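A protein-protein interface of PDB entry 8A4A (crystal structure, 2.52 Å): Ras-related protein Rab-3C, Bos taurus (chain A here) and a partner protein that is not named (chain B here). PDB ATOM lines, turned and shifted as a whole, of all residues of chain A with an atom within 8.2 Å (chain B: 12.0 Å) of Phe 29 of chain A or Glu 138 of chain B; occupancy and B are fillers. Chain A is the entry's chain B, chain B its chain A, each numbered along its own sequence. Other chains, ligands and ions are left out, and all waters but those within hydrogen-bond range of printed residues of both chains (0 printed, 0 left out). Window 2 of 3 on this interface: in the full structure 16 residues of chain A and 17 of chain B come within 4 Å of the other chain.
The side-chain hydroxyl (OG) of Ser 135 of chain B lies within hydrogen-bond range of the guanidinium group (NH1) of Arg 136 of chain B, 3.5 Å away. The backbone carbonyl oxygen (O) of Tyr 31 of chain A is in hydrogen-bond range of the backbone NH (N) of Lys 82 of chain A. The backbone carbonyl oxygen (O) of Lys 82 of chain A is in hydrogen-bond range of the backbone NH (N) of Phe 33 of chain A (2.9 Å). N of Gln 84 of chain A is in hydrogen-bond range of O of Phe 33 of chain A (2.9 Å).
The backbone carbonyl oxygen (O) of Phe 69 of chain A lies within hydrogen-bond range of a ring nitrogen (ND1) of His 86 of chain B. The backbone carbonyl oxygen (O) of Arg 136 of chain B is in hydrogen-bond range of the side-chain amino group (NZ) of Lys 82 of chain A.
Of the 15 printed residues of chain B, 4 touch a printed residue of chain A. Among the printed residues, 10 pairs touch across the chains.
No residue of chain B comes within 4 Å of Asn 28 of chain A. No residue of chain B comes within 4 Å of Asp 30 of chain A. Arg 80 of chain A touches none of the printed residues of chain B. Of chain B, only Arg 136 (3.2 Å) and Val 137 (3.9 Å) come within 4 Å of Lys 82 of chain A. Printed residues of chain B within 4 Å of Gln 84 of chain A: Arg 136 and Val 137. Of the printed residues of chain A, Val 137 of chain B touches Phe 69 (3.8 Å), Lys 82 (3.9 Å) and Gln 84 (3.6 Å). Of chain A, only Phe 29 and Met 32 come within 4 Å of Glu 138 of chain B.
Among the printed residues, pairs that only touch across the chains: Phe 29 of chain A with Glu 138 of chain B (3.3 Å), Met 32 of chain A with Glu 138 of chain B (3.6 Å), Phe 69 of chain A with Arg 136 of chain B (3.9 Å), Phe 69 of chain A with Val 137 of chain B (3.8 Å), Val 71 of chain A with Arg 136 of chain B (3.5 Å), Lys 82 of chain A with Val 137 of chain B (3.9 Å), Gln 84 of chain A with Arg 136 of chain B (3.5 Å) and Gln 84 of chain A with Val 137 of chain B (3.6 Å).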
ATOM      1  N   ASN A  28       2.116 -20.073 -25.397  1.00  0.00           N
ATOM      2  CA  ASN A  28       1.578 -19.751 -24.092  1.00  0.00           C
ATOM      3  C   ASN A  28       1.939 -18.321 -23.716  1.00  0.00           C
ATOM      4  O   ASN A  28       2.269 -18.041 -22.569  1.00  0.00           O
ATOM      5  CB  ASN A  28       2.095 -20.739 -23.048  1.00  0.00           C
ATOM      6  CG  ASN A  28       3.606 -20.766 -22.974  1.00  0.00           C
ATOM      7  OD1 ASN A  28       4.291 -20.565 -23.978  1.00  0.00           O
ATOM      8  ND2 ASN A  28       4.139 -21.011 -21.780  1.00  0.00           N
ATOM      9  N   PHE A  29       1.911 -17.421 -24.698  1.00  0.00           N
ATOM     10  CA  PHE A  29       1.951 -15.990 -24.437  1.00  0.00           C
ATOM     11  C   PHE A  29       0.926 -15.308 -25.331  1.00  0.00           C
ATOM     12  O   PHE A  29       0.652 -15.762 -26.447  1.00  0.00           O
ATOM     13  CB  PHE A  29       3.382 -15.388 -24.624  1.00  0.00           C
ATOM     14  CG  PHE A  29       3.935 -15.464 -26.038  1.00  0.00           C
ATOM     15  CD1 PHE A  29       3.407 -14.698 -27.071  1.00  0.00           C
ATOM     16  CD2 PHE A  29       5.024 -16.278 -26.316  1.00  0.00           C
ATOM     17  CE1 PHE A  29       3.930 -14.771 -28.356  1.00  0.00           C
ATOM     18  CE2 PHE A  29       5.555 -16.353 -27.599  1.00  0.00           C
ATOM     19  CZ  PHE A  29       5.006 -15.599 -28.619  1.00  0.00           C
ATOM     20  N   ASP A  30       0.326 -14.229 -24.827  1.00  0.00           N
ATOM     21  CA  ASP A  30      -0.608 -13.499 -25.676  1.00  0.00           C
ATOM     22  C   ASP A  30       0.109 -12.468 -26.539  1.00  0.00           C
ATOM     23  O   ASP A  30      -0.250 -12.278 -27.705  1.00  0.00           O
ATOM     24  CB  ASP A  30      -1.703 -12.838 -24.838  1.00  0.00           C
ATOM     25  CG  ASP A  30      -2.149 -13.700 -23.679  1.00  0.00           C
ATOM     26  OD1 ASP A  30      -2.855 -14.694 -23.927  1.00  0.00           O
ATOM     27  OD2 ASP A  30      -1.810 -13.387 -22.530  1.00  0.00           O
ATOM     28  N   TYR A  31       1.135 -11.803 -26.009  1.00  0.00           N
ATOM     29  CA  TYR A  31       1.868 -10.854 -26.842  1.00  0.00           C
ATOM     30  C   TYR A  31       3.363 -11.029 -26.629  1.00  0.00           C
ATOM     31  O   TYR A  31       3.806 -11.594 -25.628  1.00  0.00           O
ATOM     32  CB  TYR A  31       1.457  -9.399 -26.559  1.00  0.00           C
ATOM     33  CG  TYR A  31      -0.004  -9.086 -26.823  1.00  0.00           C
ATOM     34  CD1 TYR A  31      -0.573  -9.305 -28.074  1.00  0.00           C
ATOM     35  CD2 TYR A  31      -0.814  -8.583 -25.815  1.00  0.00           C
ATOM     36  CE1 TYR A  31      -1.913  -9.027 -28.310  1.00  0.00           C
ATOM     37  CE2 TYR A  31      -2.150  -8.302 -26.042  1.00  0.00           C
ATOM     38  CZ  TYR A  31      -2.695  -8.525 -27.290  1.00  0.00           C
ATOM     39  OH  TYR A  31      -4.024  -8.244 -27.516  1.00  0.00           O
ATOM     40  N   MET A  32       4.139 -10.548 -27.599  1.00  0.00           N
ATOM     41  CA  MET A  32       5.591 -10.482 -27.479  1.00  0.00           C
ATOM     42  C   MET A  32       6.048  -9.080 -27.850  1.00  0.00           C
ATOM     43  O   MET A  32       5.805  -8.621 -28.969  1.00  0.00           O
ATOM     44  CB  MET A  32       6.278 -11.515 -28.371  1.00  0.00           C
ATOM     45  CG  MET A  32       7.718 -11.773 -27.988  1.00  0.00           C
ATOM     46  SD  MET A  32       8.765 -11.971 -29.434  1.00  0.00           S
ATOM     47  CE  MET A  32      10.197 -12.769 -28.714  1.00  0.00           C
ATOM     48  N   PHE A  33       6.714  -8.410 -26.915  1.00  0.00           N
ATOM     49  CA  PHE A  33       7.229  -7.062 -27.118  1.00  0.00           C
ATOM     50  C   PHE A  33       8.747  -7.099 -27.229  1.00  0.00           C
ATOM     51  O   PHE A  33       9.428  -7.625 -26.340  1.00  0.00           O
ATOM     52  CB  PHE A  33       6.812  -6.133 -25.976  1.00  0.00           C
ATOM     53  CG  PHE A  33       5.332  -5.891 -25.895  1.00  0.00           C
ATOM     54  CD1 PHE A  33       4.512  -6.131 -26.987  1.00  0.00           C
ATOM     55  CD2 PHE A  33       4.759  -5.416 -24.724  1.00  0.00           C
ATOM     56  CE1 PHE A  33       3.151  -5.907 -26.913  1.00  0.00           C
ATOM     57  CE2 PHE A  33       3.396  -5.190 -24.643  1.00  0.00           C
ATOM     58  CZ  PHE A  33       2.590  -5.437 -25.741  1.00  0.00           C
ATOM     59  N   PHE A  69      20.660 -10.426 -25.684  1.00  0.00           N
ATOM     60  CA  PHE A  69      19.283 -10.277 -25.235  1.00  0.00           C
ATOM     61  C   PHE A  69      18.960 -11.272 -24.131  1.00  0.00           C
ATOM     62  O   PHE A  69      19.595 -12.322 -23.997  1.00  0.00           O
ATOM     63  CB  PHE A  69      18.280 -10.428 -26.390  1.00  0.00           C
ATOM     64  CG  PHE A  69      18.103 -11.847 -26.883  1.00  0.00           C
ATOM     65  CD1 PHE A  69      18.928 -12.364 -27.871  1.00  0.00           C
ATOM     66  CD2 PHE A  69      17.093 -12.651 -26.375  1.00  0.00           C
ATOM     67  CE1 PHE A  69      18.760 -13.661 -28.331  1.00  0.00           C
ATOM     68  CE2 PHE A  69      16.922 -13.952 -26.832  1.00  0.00           C
ATOM     69  CZ  PHE A  69      17.756 -14.455 -27.810  1.00  0.00           C
ATOM     70  N   VAL A  71      15.101 -12.648 -21.930  1.00  0.00           N
ATOM     71  CA  VAL A  71      13.653 -12.720 -22.074  1.00  0.00           C
ATOM     72  C   VAL A  71      13.020 -12.786 -20.693  1.00  0.00           C
ATOM     73  O   VAL A  71      13.606 -13.317 -19.746  1.00  0.00           O
ATOM     74  CB  VAL A  71      13.217 -13.927 -22.933  1.00  0.00           C
ATOM     75  CG1 VAL A  71      13.364 -13.600 -24.407  1.00  0.00           C
ATOM     76  CG2 VAL A  71      14.032 -15.151 -22.575  1.00  0.00           C
ATOM     77  N   THR A  73       8.864 -12.894 -18.755  1.00  0.00           N
ATOM     78  CA  THR A  73       7.412 -12.930 -18.881  1.00  0.00           C
ATOM     79  C   THR A  73       6.764 -12.065 -17.806  1.00  0.00           C
ATOM     80  O   THR A  73       7.132 -12.138 -16.629  1.00  0.00           O
ATOM     81  CB  THR A  73       6.894 -14.369 -18.774  1.00  0.00           C
ATOM     82  OG1 THR A  73       7.119 -15.052 -20.015  1.00  0.00           O
ATOM     83  CG2 THR A  73       5.403 -14.393 -18.446  1.00  0.00           C
ATOM     84  N   VAL A  74       5.798 -11.238 -18.218  1.00  0.00           N
ATOM     85  CA  VAL A  74       5.016 -10.415 -17.302  1.00  0.00           C
ATOM     86  C   VAL A  74       3.536 -10.572 -17.634  1.00  0.00           C
ATOM     87  O   VAL A  74       3.159 -11.131 -18.664  1.00  0.00           O
ATOM     88  CB  VAL A  74       5.420  -8.926 -17.340  1.00  0.00           C
ATOM     89  CG1 VAL A  74       6.918  -8.768 -17.144  1.00  0.00           C
ATOM     90  CG2 VAL A  74       4.980  -8.295 -18.650  1.00  0.00           C
ATOM     91  N   LYS A  79      -3.264 -10.710 -19.390  1.00  0.00           N
ATOM     92  CA  LYS A  79      -2.502 -11.021 -20.587  1.00  0.00           C
ATOM     93  C   LYS A  79      -1.071 -11.406 -20.225  1.00  0.00           C
ATOM     94  O   LYS A  79      -0.445 -10.798 -19.355  1.00  0.00           O
ATOM     95  CB  LYS A  79      -2.507  -9.838 -21.560  1.00  0.00           C
ATOM     96  CG  LYS A  79      -3.880  -9.473 -22.163  1.00  0.00           C
ATOM     97  CD  LYS A  79      -4.938 -10.581 -22.051  1.00  0.00           C
ATOM     98  CE  LYS A  79      -6.275 -10.158 -22.662  1.00  0.00           C
ATOM     99  NZ  LYS A  79      -7.369 -11.084 -22.244  1.00  0.00           N
ATOM    100  N   ARG A  80      -0.567 -12.432 -20.898  1.00  0.00           N
ATOM    101  CA  ARG A  80       0.802 -12.907 -20.740  1.00  0.00           C
ATOM    102  C   ARG A  80       1.638 -12.290 -21.857  1.00  0.00           C
ATOM    103  O   ARG A  80       1.334 -12.461 -23.051  1.00  0.00           O
ATOM    104  CB  ARG A  80       0.849 -14.438 -20.780  1.00  0.00           C
ATOM    105  CG  ARG A  80       1.872 -15.084 -19.859  1.00  0.00           C
ATOM    106  CD  ARG A  80       1.785 -16.614 -19.879  1.00  0.00           C
ATOM    107  NE  ARG A  80       0.475 -17.125 -20.274  1.00  0.00           N
ATOM    108  CZ  ARG A  80       0.209 -18.407 -20.494  1.00  0.00           C
ATOM    109  NH1 ARG A  80       1.124 -19.345 -20.311  1.00  0.00           N
ATOM    110  NH2 ARG A  80      -1.008 -18.758 -20.905  1.00  0.00           N
ATOM    111  N   ILE A  81       2.661 -11.535 -21.467  1.00  0.00           N
ATOM    112  CA  ILE A  81       3.497 -10.781 -22.389  1.00  0.00           C
ATOM    113  C   ILE A  81       4.924 -11.275 -22.223  1.00  0.00           C
ATOM    114  O   ILE A  81       5.477 -11.244 -21.114  1.00  0.00           O
ATOM    115  CB  ILE A  81       3.405  -9.269 -22.131  1.00  0.00           C
ATOM    116  CG1 ILE A  81       1.952  -8.798 -22.268  1.00  0.00           C
ATOM    117  CG2 ILE A  81       4.321  -8.509 -23.077  1.00  0.00           C
ATOM    118  CD1 ILE A  81       1.701  -7.428 -21.682  1.00  0.00           C
ATOM    119  N   LYS A  82       5.506 -11.751 -23.314  1.00  0.00           N
ATOM    120  CA  LYS A  82       6.918 -12.088 -23.356  1.00  0.00           C
ATOM    121  C   LYS A  82       7.682 -10.842 -23.781  1.00  0.00           C
ATOM    122  O   LYS A  82       7.404 -10.276 -24.843  1.00  0.00           O
ATOM    123  CB  LYS A  82       7.163 -13.238 -24.332  1.00  0.00           C
ATOM    124  CG  LYS A  82       8.550 -13.843 -24.266  1.00  0.00           C
ATOM    125  CD  LYS A  82       8.895 -14.532 -25.579  1.00  0.00           C
ATOM    126  CE  LYS A  82      10.293 -15.120 -25.544  1.00  0.00           C
ATOM    127  NZ  LYS A  82      10.467 -16.238 -26.512  1.00  0.00           N
ATOM    128  N   LEU A  83       8.630 -10.412 -22.960  1.00  0.00           N
ATOM    129  CA  LEU A  83       9.502  -9.299 -23.289  1.00  0.00           C
ATOM    130  C   LEU A  83      10.816  -9.875 -23.789  1.00  0.00           C
ATOM    131  O   LEU A  83      11.456 -10.668 -23.085  1.00  0.00           O
ATOM    132  CB  LEU A  83       9.745  -8.404 -22.072  1.00  0.00           C
ATOM    133  CG  LEU A  83       8.521  -7.979 -21.261  1.00  0.00           C
ATOM    134  CD1 LEU A  83       8.945  -7.337 -19.948  1.00  0.00           C
ATOM    135  CD2 LEU A  83       7.637  -7.037 -22.063  1.00  0.00           C
ATOM    136  N   GLN A  84      11.196  -9.500 -25.006  1.00  0.00           N
ATOM    137  CA  GLN A  84      12.512  -9.806 -25.551  1.00  0.00           C
ATOM    138  C   GLN A  84      13.320  -8.518 -25.451  1.00  0.00           C
ATOM    139  O   GLN A  84      13.154  -7.602 -26.263  1.00  0.00           O
ATOM    140  CB  GLN A  84      12.405 -10.313 -26.983  1.00  0.00           C
ATOM    141  CG  GLN A  84      13.646 -11.014 -27.487  1.00  0.00           C
ATOM    142  CD  GLN A  84      13.575 -11.311 -28.971  1.00  0.00           C
ATOM    143  OE1 GLN A  84      13.405 -10.404 -29.788  1.00  0.00           O
ATOM    144  NE2 GLN A  84      13.686 -12.588 -29.326  1.00  0.00           N
ATOM    145  N   HIS B  86      23.338 -17.071 -26.791  1.00  0.00           N
ATOM    146  CA  HIS B  86      22.568 -16.213 -27.684  1.00  0.00           C
ATOM    147  C   HIS B  86      23.475 -15.532 -28.702  1.00  0.00           C
ATOM    148  O   HIS B  86      23.142 -15.451 -29.890  1.00  0.00           O
ATOM    149  CB  HIS B  86      21.805 -15.171 -26.869  1.00  0.00           C
ATOM    150  CG  HIS B  86      20.646 -15.733 -26.105  1.00  0.00           C
ATOM    151  ND1 HIS B  86      20.030 -15.047 -25.081  1.00  0.00           N
ATOM    152  CD2 HIS B  86      19.997 -16.917 -26.208  1.00  0.00           C
ATOM    153  CE1 HIS B  86      19.047 -15.782 -24.590  1.00  0.00           C
ATOM    154  NE2 HIS B  86      19.007 -16.921 -25.256  1.00  0.00           N
ATOM    155  N   PHE B  89      24.724 -17.970 -31.351  1.00  0.00           N
ATOM    156  CA  PHE B  89      23.669 -18.186 -32.334  1.00  0.00           C
ATOM    157  C   PHE B  89      23.557 -17.009 -33.299  1.00  0.00           C
ATOM    158  O   PHE B  89      23.583 -17.192 -34.521  1.00  0.00           O
ATOM    159  CB  PHE B  89      22.335 -18.427 -31.630  1.00  0.00           C
ATOM    160  CG  PHE B  89      21.213 -18.733 -32.572  1.00  0.00           C
ATOM    161  CD1 PHE B  89      21.072 -19.999 -33.110  1.00  0.00           C
ATOM    162  CD2 PHE B  89      20.309 -17.750 -32.937  1.00  0.00           C
ATOM    163  CE1 PHE B  89      20.048 -20.284 -33.987  1.00  0.00           C
ATOM    164  CE2 PHE B  89      19.281 -18.028 -33.814  1.00  0.00           C
ATOM    165  CZ  PHE B  89      19.150 -19.298 -34.339  1.00  0.00           C
ATOM    166  N   LEU B  90      23.441 -15.788 -32.768  1.00  0.00           N
ATOM    167  CA  LEU B  90      23.163 -14.631 -33.619  1.00  0.00           C
ATOM    168  C   LEU B  90      24.319 -14.325 -34.562  1.00  0.00           C
ATOM    169  O   LEU B  90      24.100 -13.979 -35.729  1.00  0.00           O
ATOM    170  CB  LEU B  90      22.862 -13.404 -32.758  1.00  0.00           C
ATOM    171  CG  LEU B  90      21.490 -13.338 -32.091  1.00  0.00           C
ATOM    172  CD1 LEU B  90      21.513 -12.288 -31.006  1.00  0.00           C
ATOM    173  CD2 LEU B  90      20.401 -13.040 -33.106  1.00  0.00           C
ATOM    174  N   PRO B 133      17.760 -24.388 -31.422  1.00  0.00           N
ATOM    175  CA  PRO B 133      19.091 -23.838 -31.146  1.00  0.00           C
ATOM    176  C   PRO B 133      19.049 -22.468 -30.467  1.00  0.00           C
ATOM    177  O   PRO B 133      19.947 -22.152 -29.689  1.00  0.00           O
ATOM    178  CB  PRO B 133      19.717 -23.750 -32.538  1.00  0.00           C
ATOM    179  CG  PRO B 133      19.099 -24.892 -33.276  1.00  0.00           C
ATOM    180  CD  PRO B 133      17.683 -24.998 -32.761  1.00  0.00           C
ATOM    181  N   GLU B 134      18.018 -21.671 -30.756  1.00  0.00           N
ATOM    182  CA  GLU B 134      17.845 -20.358 -30.143  1.00  0.00           C
ATOM    183  C   GLU B 134      16.897 -20.399 -28.948  1.00  0.00           C
ATOM    184  O   GLU B 134      17.228 -19.882 -27.878  1.00  0.00           O
ATOM    185  CB  GLU B 134      17.365 -19.343 -31.198  1.00  0.00           C
ATOM    186  CG  GLU B 134      15.906 -19.455 -31.669  1.00  0.00           C
ATOM    187  CD  GLU B 134      15.676 -20.573 -32.675  1.00  0.00           C
ATOM    188  OE1 GLU B 134      16.568 -21.430 -32.841  1.00  0.00           O
ATOM    189  OE2 GLU B 134      14.594 -20.589 -33.303  1.00  0.00           O
ATOM    190  N   SER B 135      15.709 -20.979 -29.127  1.00  0.00           N
ATOM    191  CA  SER B 135      14.773 -21.398 -28.086  1.00  0.00           C
ATOM    192  C   SER B 135      14.090 -20.248 -27.354  1.00  0.00           C
ATOM    193  O   SER B 135      13.078 -20.468 -26.683  1.00  0.00           O
ATOM    194  CB  SER B 135      15.471 -22.299 -27.056  1.00  0.00           C
ATOM    195  OG  SER B 135      16.502 -21.616 -26.362  1.00  0.00           O
ATOM    196  N   ARG B 136      14.565 -19.019 -27.532  1.00  0.00           N
ATOM    197  CA  ARG B 136      14.013 -17.864 -26.834  1.00  0.00           C
ATOM    198  C   ARG B 136      13.561 -16.808 -27.833  1.00  0.00           C
ATOM    199  O   ARG B 136      13.489 -15.619 -27.515  1.00  0.00           O
ATOM    200  CB  ARG B 136      15.024 -17.285 -25.843  1.00  0.00           C
ATOM    201  CG  ARG B 136      15.588 -18.291 -24.837  1.00  0.00           C
ATOM    202  CD  ARG B 136      14.698 -18.454 -23.603  1.00  0.00           C
ATOM    203  NE  ARG B 136      13.455 -19.165 -23.875  1.00  0.00           N
ATOM    204  CZ  ARG B 136      13.334 -20.485 -23.892  1.00  0.00           C
ATOM    205  NH1 ARG B 136      14.365 -21.277 -23.647  1.00  0.00           N
ATOM    206  NH2 ARG B 136      12.152 -21.026 -24.180  1.00  0.00           N
ATOM    207  N   VAL B 137      13.254 -17.246 -29.050  1.00  0.00           N
ATOM    208  CA  VAL B 137      12.901 -16.365 -30.152  1.00  0.00           C
ATOM    209  C   VAL B 137      11.659 -16.932 -30.821  1.00  0.00           C
ATOM    210  O   VAL B 137      11.580 -18.142 -31.063  1.00  0.00           O
ATOM    211  CB  VAL B 137      14.056 -16.238 -31.166  1.00  0.00           C
ATOM    212  CG1 VAL B 137      13.626 -15.417 -32.350  1.00  0.00           C
ATOM    213  CG2 VAL B 137      15.288 -15.627 -30.512  1.00  0.00           C
ATOM    214  N   GLU B 138      10.679 -16.073 -31.093  1.00  0.00           N
ATOM    215  CA  GLU B 138       9.529 -16.496 -31.873  1.00  0.00           C
ATOM    216  C   GLU B 138       9.866 -16.423 -33.363  1.00  0.00           C
ATOM    217  O   GLU B 138      10.942 -15.970 -33.759  1.00  0.00           O
ATOM    218  CB  GLU B 138       8.304 -15.648 -31.530  1.00  0.00           C
ATOM    219  CG  GLU B 138       8.262 -14.285 -32.195  1.00  0.00           C
ATOM    220  CD  GLU B 138       6.852 -13.720 -32.266  1.00  0.00           C
ATOM    221  OE1 GLU B 138       6.078 -13.927 -31.306  1.00  0.00           O
ATOM    222  OE2 GLU B 138       6.520 -13.073 -33.282  1.00  0.00           O
ATOM    223  N   GLU B 139       8.927 -16.873 -34.198  1.00  0.00           N
ATOM    224  CA  GLU B 139       9.227 -17.137 -35.604  1.00  0.00           C
ATOM    225  C   GLU B 139       9.788 -15.922 -36.336  1.00  0.00           C
ATOM    226  O   GLU B 139       9.085 -14.930 -36.555  1.00  0.00           O
ATOM    227  CB  GLU B 139       7.980 -17.645 -36.331  1.00  0.00           C
ATOM    228  CG  GLU B 139       8.282 -18.263 -37.690  1.00  0.00           C
ATOM    229  CD  GLU B 139       7.186 -19.192 -38.172  1.00  0.00           C
ATOM    230  OE1 GLU B 139       5.996 -18.844 -38.016  1.00  0.00           O
ATOM    231  OE2 GLU B 139       7.514 -20.272 -38.707  1.00  0.00           O
ATOM    232  N   SER B 140      11.064 -16.011 -36.717  1.00  0.00           N
ATOM    233  CA  SER B 140      11.731 -15.000 -37.528  1.00  0.00           C
ATOM    234  C   SER B 140      12.473 -15.681 -38.670  1.00  0.00           C
ATOM    235  O   SER B 140      12.388 -16.904 -38.825  1.00  0.00           O
ATOM    236  CB  SER B 140      12.698 -14.171 -36.682  1.00  0.00           C
ATOM    237  OG  SER B 140      13.197 -13.058 -37.403  1.00  0.00           O
ATOM    238  N   SER B 141      13.199 -14.913 -39.472  1.00  0.00           N
ATOM    239  CA  SER B 141      14.020 -15.483 -40.542  1.00  0.00           C
ATOM    240  C   SER B 141      15.438 -15.772 -40.058  1.00  0.00           C
ATOM    241  O   SER B 141      16.419 -15.353 -40.673  1.00  0.00           O
ATOM    242  CB  SER B 141      14.028 -14.549 -41.749  1.00  0.00           C
ATOM    243  OG  SER B 141      14.453 -13.246 -41.383  1.00  0.00           O
ATOM    244  N   TRP B 142      15.571 -16.508 -38.952  1.00  0.00           N
ATOM    245  CA  TRP B 142      16.872 -16.910 -38.429  1.00  0.00           C
ATOM    246  C   TRP B 142      17.199 -18.365 -38.741  1.00  0.00           C
ATOM    247  O   TRP B 142      17.852 -19.043 -37.937  1.00  0.00           O
ATOM    248  CB  TRP B 142      16.951 -16.659 -36.924  1.00  0.00           C
ATOM    249  CG  TRP B 142      17.490 -15.304 -36.573  1.00  0.00           C
ATOM    250  CD1 TRP B 142      18.644 -14.735 -37.035  1.00  0.00           C
ATOM    251  CD2 TRP B 142      16.898 -14.348 -35.686  1.00  0.00           C
ATOM    252  NE1 TRP B 142      18.803 -13.482 -36.491  1.00  0.00           N
ATOM    253  CE2 TRP B 142      17.745 -13.222 -35.659  1.00  0.00           C
ATOM    254  CE3 TRP B 142      15.735 -14.335 -34.914  1.00  0.00           C
ATOM    255  CZ2 TRP B 142      17.463 -12.095 -34.891  1.00  0.00           C
ATOM    256  CZ3 TRP B 142      15.457 -13.214 -34.153  1.00  0.00           C
ATOM    257  CH2 TRP B 142      16.318 -12.113 -34.146  1.00  0.00           C
ATOM    258  N   LYS B 143      16.754 -18.863 -39.896  1.00  0.00           N
ATOM    259  CA  LYS B 143      17.169 -20.163 -40.402  1.00  0.00           C
ATOM    260  C   LYS B 143      18.420 -20.059 -41.268  1.00  0.00           C
ATOM    261  O   LYS B 143      18.648 -20.913 -42.133  1.00  0.00           O
ATOM    262  CB  LYS B 143      16.023 -20.815 -41.178  1.00  0.00           C
ATOM    263  CG  LYS B 143      14.928 -21.394 -40.283  1.00  0.00           C
ATOM    264  CD  LYS B 143      15.513 -21.996 -39.009  1.00  0.00           C
ATOM    265  CE  LYS B 143      14.444 -22.661 -38.150  1.00  0.00           C
ATOM    266  NZ  LYS B 143      13.413 -21.682 -37.697  1.00  0.00           N
ATOM    267  N   LYS B 144      19.219 -19.018 -41.056  1.00  0.00           N
ATOM    268  CA  LYS B 144      20.458 -18.806 -41.783  1.00  0.00           C
ATOM    269  C   LYS B 144      21.566 -19.661 -41.179  1.00  0.00           C
ATOM    270  O   LYS B 144      21.569 -19.948 -39.978  1.00  0.00           O
ATOM    271  CB  LYS B 144      20.825 -17.321 -41.736  1.00  0.00           C
ATOM    272  CG  LYS B 144      21.696 -16.832 -42.869  1.00  0.00           C
ATOM    273  CD  LYS B 144      22.091 -15.377 -42.650  1.00  0.00           C
ATOM    274  CE  LYS B 144      20.881 -14.467 -42.782  1.00  0.00           C
ATOM    275  NZ  LYS B 144      21.232 -13.031 -42.630  1.00  0.00           N
